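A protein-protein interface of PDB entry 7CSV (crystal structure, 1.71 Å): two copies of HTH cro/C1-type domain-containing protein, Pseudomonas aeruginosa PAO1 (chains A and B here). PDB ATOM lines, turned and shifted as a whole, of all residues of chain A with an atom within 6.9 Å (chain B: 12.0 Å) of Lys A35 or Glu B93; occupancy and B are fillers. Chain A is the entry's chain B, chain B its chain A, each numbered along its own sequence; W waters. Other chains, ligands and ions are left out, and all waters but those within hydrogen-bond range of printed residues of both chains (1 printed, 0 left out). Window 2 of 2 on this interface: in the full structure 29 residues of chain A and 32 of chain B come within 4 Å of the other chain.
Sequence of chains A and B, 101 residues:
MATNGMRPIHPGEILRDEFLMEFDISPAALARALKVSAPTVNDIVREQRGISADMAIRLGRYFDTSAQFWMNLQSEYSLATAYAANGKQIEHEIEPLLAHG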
ATOM      1  N   LEU A  30       9.047  16.148  13.718  1.00  0.00           N
ATOM      2  CA  LEU A  30       9.032  14.943  12.898  1.00  0.00           C
ATOM      3  C   LEU A  30       9.884  13.848  13.523  1.00  0.00           C
ATOM      4  O   LEU A  30       9.459  12.688  13.604  1.00  0.00           O
ATOM      5  CB  LEU A  30       9.518  15.267  11.481  1.00  0.00           C
ATOM      6  CG  LEU A  30       9.657  14.039  10.577  1.00  0.00           C
ATOM      7  CD1 LEU A  30       8.306  13.346  10.367  1.00  0.00           C
ATOM      8  CD2 LEU A  30      10.312  14.392   9.229  1.00  0.00           C
ATOM      9  N   ALA A  31      11.083  14.204  13.995  1.00  0.00           N
ATOM     10  CA  ALA A  31      11.964  13.220  14.611  1.00  0.00           C
ATOM     11  C   ALA A  31      11.297  12.553  15.806  1.00  0.00           C
ATOM     12  O   ALA A  31      11.382  11.329  15.974  1.00  0.00           O
ATOM     13  CB  ALA A  31      13.277  13.881  15.032  1.00  0.00           C
ATOM     14  N   ARG A  32      10.618  13.340  16.645  1.00  0.00           N
ATOM     15  CA  ARG A  32       9.941  12.763  17.802  1.00  0.00           C
ATOM     16  C   ARG A  32       8.827  11.821  17.375  1.00  0.00           C
ATOM     17  O   ARG A  32       8.622  10.770  17.994  1.00  0.00           O
ATOM     18  CB  ARG A  32       9.394  13.876  18.693  1.00  0.00           C
ATOM     19  CG  ARG A  32      10.482  14.654  19.414  1.00  0.00           C
ATOM     20  CD  ARG A  32       9.914  15.466  20.565  1.00  0.00           C
ATOM     21  NE  ARG A  32       8.895  16.406  20.113  1.00  0.00           N
ATOM     22  CZ  ARG A  32       9.144  17.657  19.746  1.00  0.00           C
ATOM     23  NH1 ARG A  32      10.389  18.119  19.772  1.00  0.00           N
ATOM     24  NH2 ARG A  32       8.151  18.443  19.352  1.00  0.00           N
ATOM     25  N   ALA A  33       8.102  12.172  16.312  1.00  0.00           N
ATOM     26  CA  ALA A  33       7.038  11.301  15.827  1.00  0.00           C
ATOM     27  C   ALA A  33       7.606  10.027  15.220  1.00  0.00           C
ATOM     28  O   ALA A  33       7.007   8.954  15.340  1.00  0.00           O
ATOM     29  CB  ALA A  33       6.179  12.044  14.800  1.00  0.00           C
ATOM     30  N   LEU A  34       8.759  10.131  14.550  1.00  0.00           N
ATOM     31  CA  LEU A  34       9.382   8.972  13.928  1.00  0.00           C
ATOM     32  C   LEU A  34      10.192   8.140  14.911  1.00  0.00           C
ATOM     33  O   LEU A  34      10.632   7.047  14.545  1.00  0.00           O
ATOM     34  CB  LEU A  34      10.292   9.411  12.785  1.00  0.00           C
ATOM     35  CG  LEU A  34       9.683  10.212  11.640  1.00  0.00           C
ATOM     36  CD1 LEU A  34      10.772  10.532  10.622  1.00  0.00           C
ATOM     37  CD2 LEU A  34       8.544   9.453  10.991  1.00  0.00           C
ATOM     38  N   LYS A  35      10.401   8.637  16.132  1.00  0.00           N
ATOM     39  CA  LYS A  35      11.186   7.942  17.151  1.00  0.00           C
ATOM     40  C   LYS A  35      12.640   7.768  16.705  1.00  0.00           C
ATOM     41  O   LYS A  35      13.237   6.702  16.865  1.00  0.00           O
ATOM     42  CB  LYS A  35      10.552   6.596  17.522  1.00  0.00           C
ATOM     43  CG  LYS A  35       9.078   6.697  17.942  1.00  0.00           C
ATOM     44  CD  LYS A  35       8.899   7.663  19.103  1.00  0.00           C
ATOM     45  CE  LYS A  35       7.449   8.116  19.306  1.00  0.00           C
ATOM     46  NZ  LYS A  35       6.459   7.026  19.436  1.00  0.00           N
ATOM     47  N   VAL A  36      13.205   8.833  16.123  1.00  0.00           N
ATOM     48  CA  VAL A  36      14.610   8.904  15.744  1.00  0.00           C
ATOM     49  C   VAL A  36      15.198  10.156  16.379  1.00  0.00           C
ATOM     50  O   VAL A  36      14.483  11.087  16.754  1.00  0.00           O
ATOM     51  CB  VAL A  36      14.830   8.936  14.208  1.00  0.00           C
ATOM     52  CG1 VAL A  36      14.328   7.661  13.566  1.00  0.00           C
ATOM     53  CG2 VAL A  36      14.150  10.147  13.590  1.00  0.00           C
ATOM     54  N   SER A  37      16.524  10.179  16.482  1.00  0.00           N
ATOM     55  CA  SER A  37      17.187  11.343  17.050  1.00  0.00           C
ATOM     56  C   SER A  37      16.994  12.553  16.139  1.00  0.00           C
ATOM     57  O   SER A  37      16.850  12.427  14.918  1.00  0.00           O
ATOM     58  CB  SER A  37      18.676  11.064  17.262  1.00  0.00           C
ATOM     59  OG  SER A  37      19.379  11.178  16.038  1.00  0.00           O
ATOM     60  N   ARG A  58      10.096   4.529   8.075  1.00  0.00           N
ATOM     61  CA  ARG A  58       9.508   5.423   9.067  1.00  0.00           C
ATOM     62  C   ARG A  58       8.764   6.570   8.402  1.00  0.00           C
ATOM     63  O   ARG A  58       7.642   6.899   8.794  1.00  0.00           O
ATOM     64  CB  ARG A  58      10.588   5.950  10.008  1.00  0.00           C
ATOM     65  CG  ARG A  58      11.313   4.840  10.763  1.00  0.00           C
ATOM     66  CD  ARG A  58      12.305   5.401  11.773  1.00  0.00           C
ATOM     67  NE  ARG A  58      12.948   4.325  12.524  1.00  0.00           N
ATOM     68  CZ  ARG A  58      12.480   3.818  13.664  1.00  0.00           C
ATOM     69  NH1 ARG A  58      11.375   4.302  14.215  1.00  0.00           N
ATOM     70  NH2 ARG A  58      13.128   2.838  14.265  1.00  0.00           N
ATOM     71  N   ARG A  61       5.549   5.205   6.819  1.00  0.00           N
ATOM     72  CA  ARG A  61       4.565   4.945   7.866  1.00  0.00           C
ATOM     73  C   ARG A  61       3.884   6.230   8.317  1.00  0.00           C
ATOM     74  O   ARG A  61       2.651   6.299   8.422  1.00  0.00           O
ATOM     75  CB  ARG A  61       5.249   4.263   9.050  1.00  0.00           C
ATOM     76  CG  ARG A  61       4.375   4.160  10.297  1.00  0.00           C
ATOM     77  CD  ARG A  61       3.337   3.090  10.167  1.00  0.00           C
ATOM     78  NE  ARG A  61       2.648   2.851  11.442  1.00  0.00           N
ATOM     79  CZ  ARG A  61       1.511   2.176  11.545  1.00  0.00           C
ATOM     80  NH1 ARG A  61       0.943   2.004  12.732  1.00  0.00           N
ATOM     81  NH2 ARG A  61       0.939   1.677  10.454  1.00  0.00           N
ATOM     82  N   ALA B  82      15.438  -4.478   5.822  1.00  0.00           N
ATOM     83  CA  ALA B  82      15.128  -3.538   6.896  1.00  0.00           C
ATOM     84  C   ALA B  82      13.752  -3.801   7.478  1.00  0.00           C
ATOM     85  O   ALA B  82      13.564  -3.721   8.700  1.00  0.00           O
ATOM     86  CB  ALA B  82      15.202  -2.099   6.384  1.00  0.00           C
ATOM     87  N   TYR B  83      12.774  -4.106   6.619  1.00  0.00           N
ATOM     88  CA  TYR B  83      11.427  -4.370   7.117  1.00  0.00           C
ATOM     89  C   TYR B  83      11.391  -5.639   7.955  1.00  0.00           C
ATOM     90  O   TYR B  83      10.741  -5.677   9.008  1.00  0.00           O
ATOM     91  CB  TYR B  83      10.425  -4.491   5.972  1.00  0.00           C
ATOM     92  CG  TYR B  83       9.003  -4.563   6.479  1.00  0.00           C
ATOM     93  CD1 TYR B  83       8.342  -3.414   6.889  1.00  0.00           C
ATOM     94  CD2 TYR B  83       8.348  -5.782   6.607  1.00  0.00           C
ATOM     95  CE1 TYR B  83       7.034  -3.470   7.379  1.00  0.00           C
ATOM     96  CE2 TYR B  83       7.043  -5.854   7.102  1.00  0.00           C
ATOM     97  CZ  TYR B  83       6.398  -4.692   7.485  1.00  0.00           C
ATOM     98  OH  TYR B  83       5.110  -4.753   7.980  1.00  0.00           O
ATOM     99  N   ALA B  85      13.629  -6.864   9.709  1.00  0.00           N
ATOM    100  CA  ALA B  85      14.340  -6.630  10.962  1.00  0.00           C
ATOM    101  C   ALA B  85      13.573  -5.688  11.890  1.00  0.00           C
ATOM    102  O   ALA B  85      13.353  -6.014  13.060  1.00  0.00           O
ATOM    103  CB  ALA B  85      15.737  -6.079  10.669  1.00  0.00           C
ATOM    104  N   ASN B  86      13.165  -4.511  11.401  1.00  0.00           N
ATOM    105  CA  ASN B  86      12.612  -3.481  12.285  1.00  0.00           C
ATOM    106  C   ASN B  86      11.214  -3.005  11.902  1.00  0.00           C
ATOM    107  O   ASN B  86      10.663  -2.139  12.603  1.00  0.00           O
ATOM    108  CB  ASN B  86      13.541  -2.259  12.333  1.00  0.00           C
ATOM    109  CG  ASN B  86      14.983  -2.626  12.633  1.00  0.00           C
ATOM    110  OD1 ASN B  86      15.254  -3.557  13.384  1.00  0.00           O
ATOM    111  ND2 ASN B  86      15.916  -1.915  12.007  1.00  0.00           N
ATOM    112  N   GLY B  87      10.623  -3.554  10.833  1.00  0.00           N
ATOM    113  CA  GLY B  87       9.367  -3.026  10.320  1.00  0.00           C
ATOM    114  C   GLY B  87       8.210  -3.167  11.293  1.00  0.00           C
ATOM    115  O   GLY B  87       7.388  -2.260  11.422  1.00  0.00           O
ATOM    116  N   LYS B  88       8.117  -4.304  11.978  1.00  0.00           N
ATOM    117  CA  LYS B  88       7.015  -4.466  12.927  1.00  0.00           C
ATOM    118  C   LYS B  88       7.128  -3.486  14.086  1.00  0.00           C
ATOM    119  O   LYS B  88       6.115  -2.919  14.522  1.00  0.00           O
ATOM    120  CB  LYS B  88       6.964  -5.899  13.441  1.00  0.00           C
ATOM    121  CG  LYS B  88       6.757  -6.919  12.343  1.00  0.00           C
ATOM    122  CD  LYS B  88       5.458  -6.686  11.606  1.00  0.00           C
ATOM    123  CE  LYS B  88       5.288  -7.727  10.509  1.00  0.00           C
ATOM    124  NZ  LYS B  88       3.858  -7.878  10.112  1.00  0.00           N
ATOM    125  N   GLN B  89       8.340  -3.293  14.614  1.00  0.00           N
ATOM    126  CA  GLN B  89       8.548  -2.302  15.669  1.00  0.00           C
ATOM    127  C   GLN B  89       8.254  -0.895  15.170  1.00  0.00           C
ATOM    128  O   GLN B  89       7.636  -0.095  15.880  1.00  0.00           O
ATOM    129  CB  GLN B  89       9.985  -2.381  16.193  1.00  0.00           C
ATOM    130  CG  GLN B  89      10.323  -1.342  17.271  1.00  0.00           C
ATOM    131  CD  GLN B  89       9.589  -1.597  18.573  1.00  0.00           C
ATOM    132  OE1 GLN B  89       9.434  -2.744  18.992  1.00  0.00           O
ATOM    133  NE2 GLN B  89       9.132  -0.529  19.220  1.00  0.00           N
ATOM    134  N   ILE B  90       8.696  -0.575  13.951  1.00  0.00           N
ATOM    135  CA  ILE B  90       8.435   0.747  13.387  1.00  0.00           C
ATOM    136  C   ILE B  90       6.937   1.004  13.315  1.00  0.00           C
ATOM    137  O   ILE B  90       6.450   2.074  13.703  1.00  0.00           O
ATOM    138  CB  ILE B  90       9.096   0.880  12.001  1.00  0.00           C
ATOM    139  CG1 ILE B  90      10.604   1.056  12.153  1.00  0.00           C
ATOM    140  CG2 ILE B  90       8.505   2.060  11.239  1.00  0.00           C
ATOM    141  CD1 ILE B  90      11.385   0.997  10.808  1.00  0.00           C
ATOM    142  N   GLU B  91       6.180   0.026  12.823  1.00  0.00           N
ATOM    143  CA  GLU B  91       4.734   0.196  12.746  1.00  0.00           C
ATOM    144  C   GLU B  91       4.106   0.252  14.127  1.00  0.00           C
ATOM    145  O   GLU B  91       3.089   0.933  14.316  1.00  0.00           O
ATOM    146  CB  GLU B  91       4.130  -0.925  11.903  1.00  0.00           C
ATOM    147  CG  GLU B  91       4.461  -0.723  10.439  1.00  0.00           C
ATOM    148  CD  GLU B  91       4.300  -1.957   9.579  1.00  0.00           C
ATOM    149  OE1 GLU B  91       4.085  -3.061  10.115  1.00  0.00           O
ATOM    150  OE2 GLU B  91       4.414  -1.802   8.347  1.00  0.00           O
ATOM    151  N   HIS B  92       4.708  -0.431  15.103  1.00  0.00           N
ATOM    152  CA  HIS B  92       4.209  -0.400  16.474  1.00  0.00           C
ATOM    153  C   HIS B  92       4.411   0.959  17.132  1.00  0.00           C
ATOM    154  O   HIS B  92       3.587   1.368  17.960  1.00  0.00           O
ATOM    155  CB  HIS B  92       4.895  -1.503  17.284  1.00  0.00           C
ATOM    156  CG  HIS B  92       4.536  -1.521  18.739  1.00  0.00           C
ATOM    157  ND1 HIS B  92       3.294  -1.899  19.201  1.00  0.00           N
ATOM    158  CD2 HIS B  92       5.275  -1.239  19.837  1.00  0.00           C
ATOM    159  CE1 HIS B  92       3.277  -1.833  20.520  1.00  0.00           C
ATOM    160  NE2 HIS B  92       4.467  -1.434  20.932  1.00  0.00           N
ATOM    161  N   GLU B  93       5.488   1.670  16.802  1.00  0.00           N
ATOM    162  CA  GLU B  93       5.823   2.871  17.553  1.00  0.00           C
ATOM    163  C   GLU B  93       5.527   4.173  16.829  1.00  0.00           C
ATOM    164  O   GLU B  93       5.600   5.229  17.460  1.00  0.00           O
ATOM    165  CB  GLU B  93       7.295   2.856  17.969  1.00  0.00           C
ATOM    166  CG  GLU B  93       8.263   2.942  16.811  1.00  0.00           C
ATOM    167  CD  GLU B  93       9.666   2.519  17.192  1.00  0.00           C
ATOM    168  OE1 GLU B  93       9.850   1.952  18.289  1.00  0.00           O
ATOM    169  OE2 GLU B  93      10.590   2.750  16.392  1.00  0.00           O
ATOM    170  N   ILE B  94       5.207   4.142  15.535  1.00  0.00           N
ATOM    171  CA  ILE B  94       4.897   5.357  14.790  1.00  0.00           C
ATOM    172  C   ILE B  94       3.405   5.375  14.493  1.00  0.00           C
ATOM    173  O   ILE B  94       2.875   4.444  13.874  1.00  0.00           O
ATOM    174  CB  ILE B  94       5.725   5.451  13.500  1.00  0.00           C
ATOM    175  CG1 ILE B  94       7.205   5.550  13.852  1.00  0.00           C
ATOM    176  CG2 ILE B  94       5.301   6.665  12.683  1.00  0.00           C
ATOM    177  CD1 ILE B  94       8.097   5.636  12.645  1.00  0.00           C
ATOM    178  N   GLU B  95       2.729   6.426  14.955  1.00  0.00           N
ATOM    179  CA  GLU B  95       1.315   6.624  14.676  1.00  0.00           C
ATOM    180  C   GLU B  95       1.183   7.476  13.425  1.00  0.00           C
ATOM    181  O   GLU B  95       1.668   8.616  13.420  1.00  0.00           O
ATOM    182  CB  GLU B  95       0.632   7.321  15.842  1.00  0.00           C
ATOM    183  CG  GLU B  95      -0.857   7.572  15.638  1.00  0.00           C
ATOM    184  CD  GLU B  95      -1.687   6.994  16.767  1.00  0.00           C
ATOM    185  OE1 GLU B  95      -2.904   7.280  16.828  1.00  0.00           O
ATOM    186  OE2 GLU B  95      -1.114   6.250  17.594  1.00  0.00           O
ATOM    187  N   PRO B  96       0.567   6.978  12.351  1.00  0.00           N
ATOM    188  CA  PRO B  96       0.503   7.769  11.113  1.00  0.00           C
ATOM    189  C   PRO B  96      -0.157   9.118  11.331  1.00  0.00           C
ATOM    190  O   PRO B  96      -1.073   9.264  12.141  1.00  0.00           O
ATOM    191  CB  PRO B  96      -0.328   6.888  10.171  1.00  0.00           C
ATOM    192  CG  PRO B  96      -0.091   5.493  10.671  1.00  0.00           C
ATOM    193  CD  PRO B  96       0.011   5.626  12.166  1.00  0.00           C
ATOM    194  N   LEU B  97       0.330  10.112  10.596  1.00  0.00           N
ATOM    195  CA  LEU B  97      -0.182  11.468  10.723  1.00  0.00           C
ATOM    196  C   LEU B  97      -1.624  11.545  10.252  1.00  0.00           C
ATOM    197  O   LEU B  97      -1.973  11.031   9.186  1.00  0.00           O
ATOM    198  CB  LEU B  97       0.675  12.436   9.906  1.00  0.00           C
ATOM    199  CG  LEU B  97       0.176  13.880   9.821  1.00  0.00           C
ATOM    200  CD1 LEU B  97       0.293  14.587  11.154  1.00  0.00           C
ATOM    201  CD2 LEU B  97       0.913  14.663   8.723  1.00  0.00           C
HETATM  202  O   HOH W   1       4.394   8.683  16.305  1.00  0.00           O
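Of the 10 printed residues of chain A, 5 touch a printed residue of chain B. Printed residues of chain A that touch a printed residue of chain B: Ala A33, Leu A34, Lys A35, Arg A58 and Arg A61. Hydrophobic or aromatic side chains of chain B that line the printed part of chain A: Ile B90, Ile B94 and Pro B96. Among the printed residues, 9 pairs touch across the chains. Among the printed residues, Asp or Glu carboxylates within 4 Å of a Lys or Arg side-chain nitrogen of the other chain: Arg A58 with Glu B93 (2.8 Å).
The backbone carbonyl oxygen (O) of Glu B91 sits at hydrogen-bond distance from the guanidinium group (NH1) of Arg A61, 2.9 Å away. The backbone carbonyl oxygen (O) of Glu B93 lies within hydrogen-bond range of the side-chain amino group (NZ) of Lys A35 (2.8 Å). NH1 of Arg A58 lies within salt-bridge range of OE2 of Glu B93. The backbone carbonyl oxygen (O) of Ile B94 is in hydrogen-bond range of the guanidinium group (NE) of Arg A61 (2.9 Å).
OH of Tyr B83 lies within hydrogen-bond range of OE1 of Glu B91 (2.9 Å). NE2 of Gln B89 sits at hydrogen-bond distance from OE1 of Glu B93. NH1 of Arg A58 sits at hydrogen-bond distance from O of Leu A34 (2.9 Å).
No position is printed for both chains.
No residue of chain B comes within 4 Å of Ala A31. Of chain B, only Ile B94 comes within 4 Å of Leu A34. Of chain B, only Glu B93 (2.8 Å) comes within 4 Å of Lys A35. No residue of chain B comes within 4 Å of Val A36. No residue of chain B comes within 4 Å of Ser A37. Of the printed residues of chain B, Arg A58 touches Ile B90 (3.7 Å), Glu B93 (2.8 Å) and Ile B94 (3.6 Å). Asn B86 touches none of the printed residues of chain A. Of the printed residues of chain A, Glu B91 touches Arg A61. Of chain A, only Lys A35 (2.8 Å) and Arg A58 (2.8 Å) come within 4 Å of Glu B93.
Water W1 lies within hydrogen-bond range of the backbone carbonyl oxygen (O) of Ala A33 and the backbone NH (N) of Glu B95.
Among the printed residues, pairs that only touch across the chains: Leu A34 with Ile B94, Arg A61 with Pro B96, Arg A58 with Ile B94, Arg A58 with Ile B90 and Ala A33 with Ile B94.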
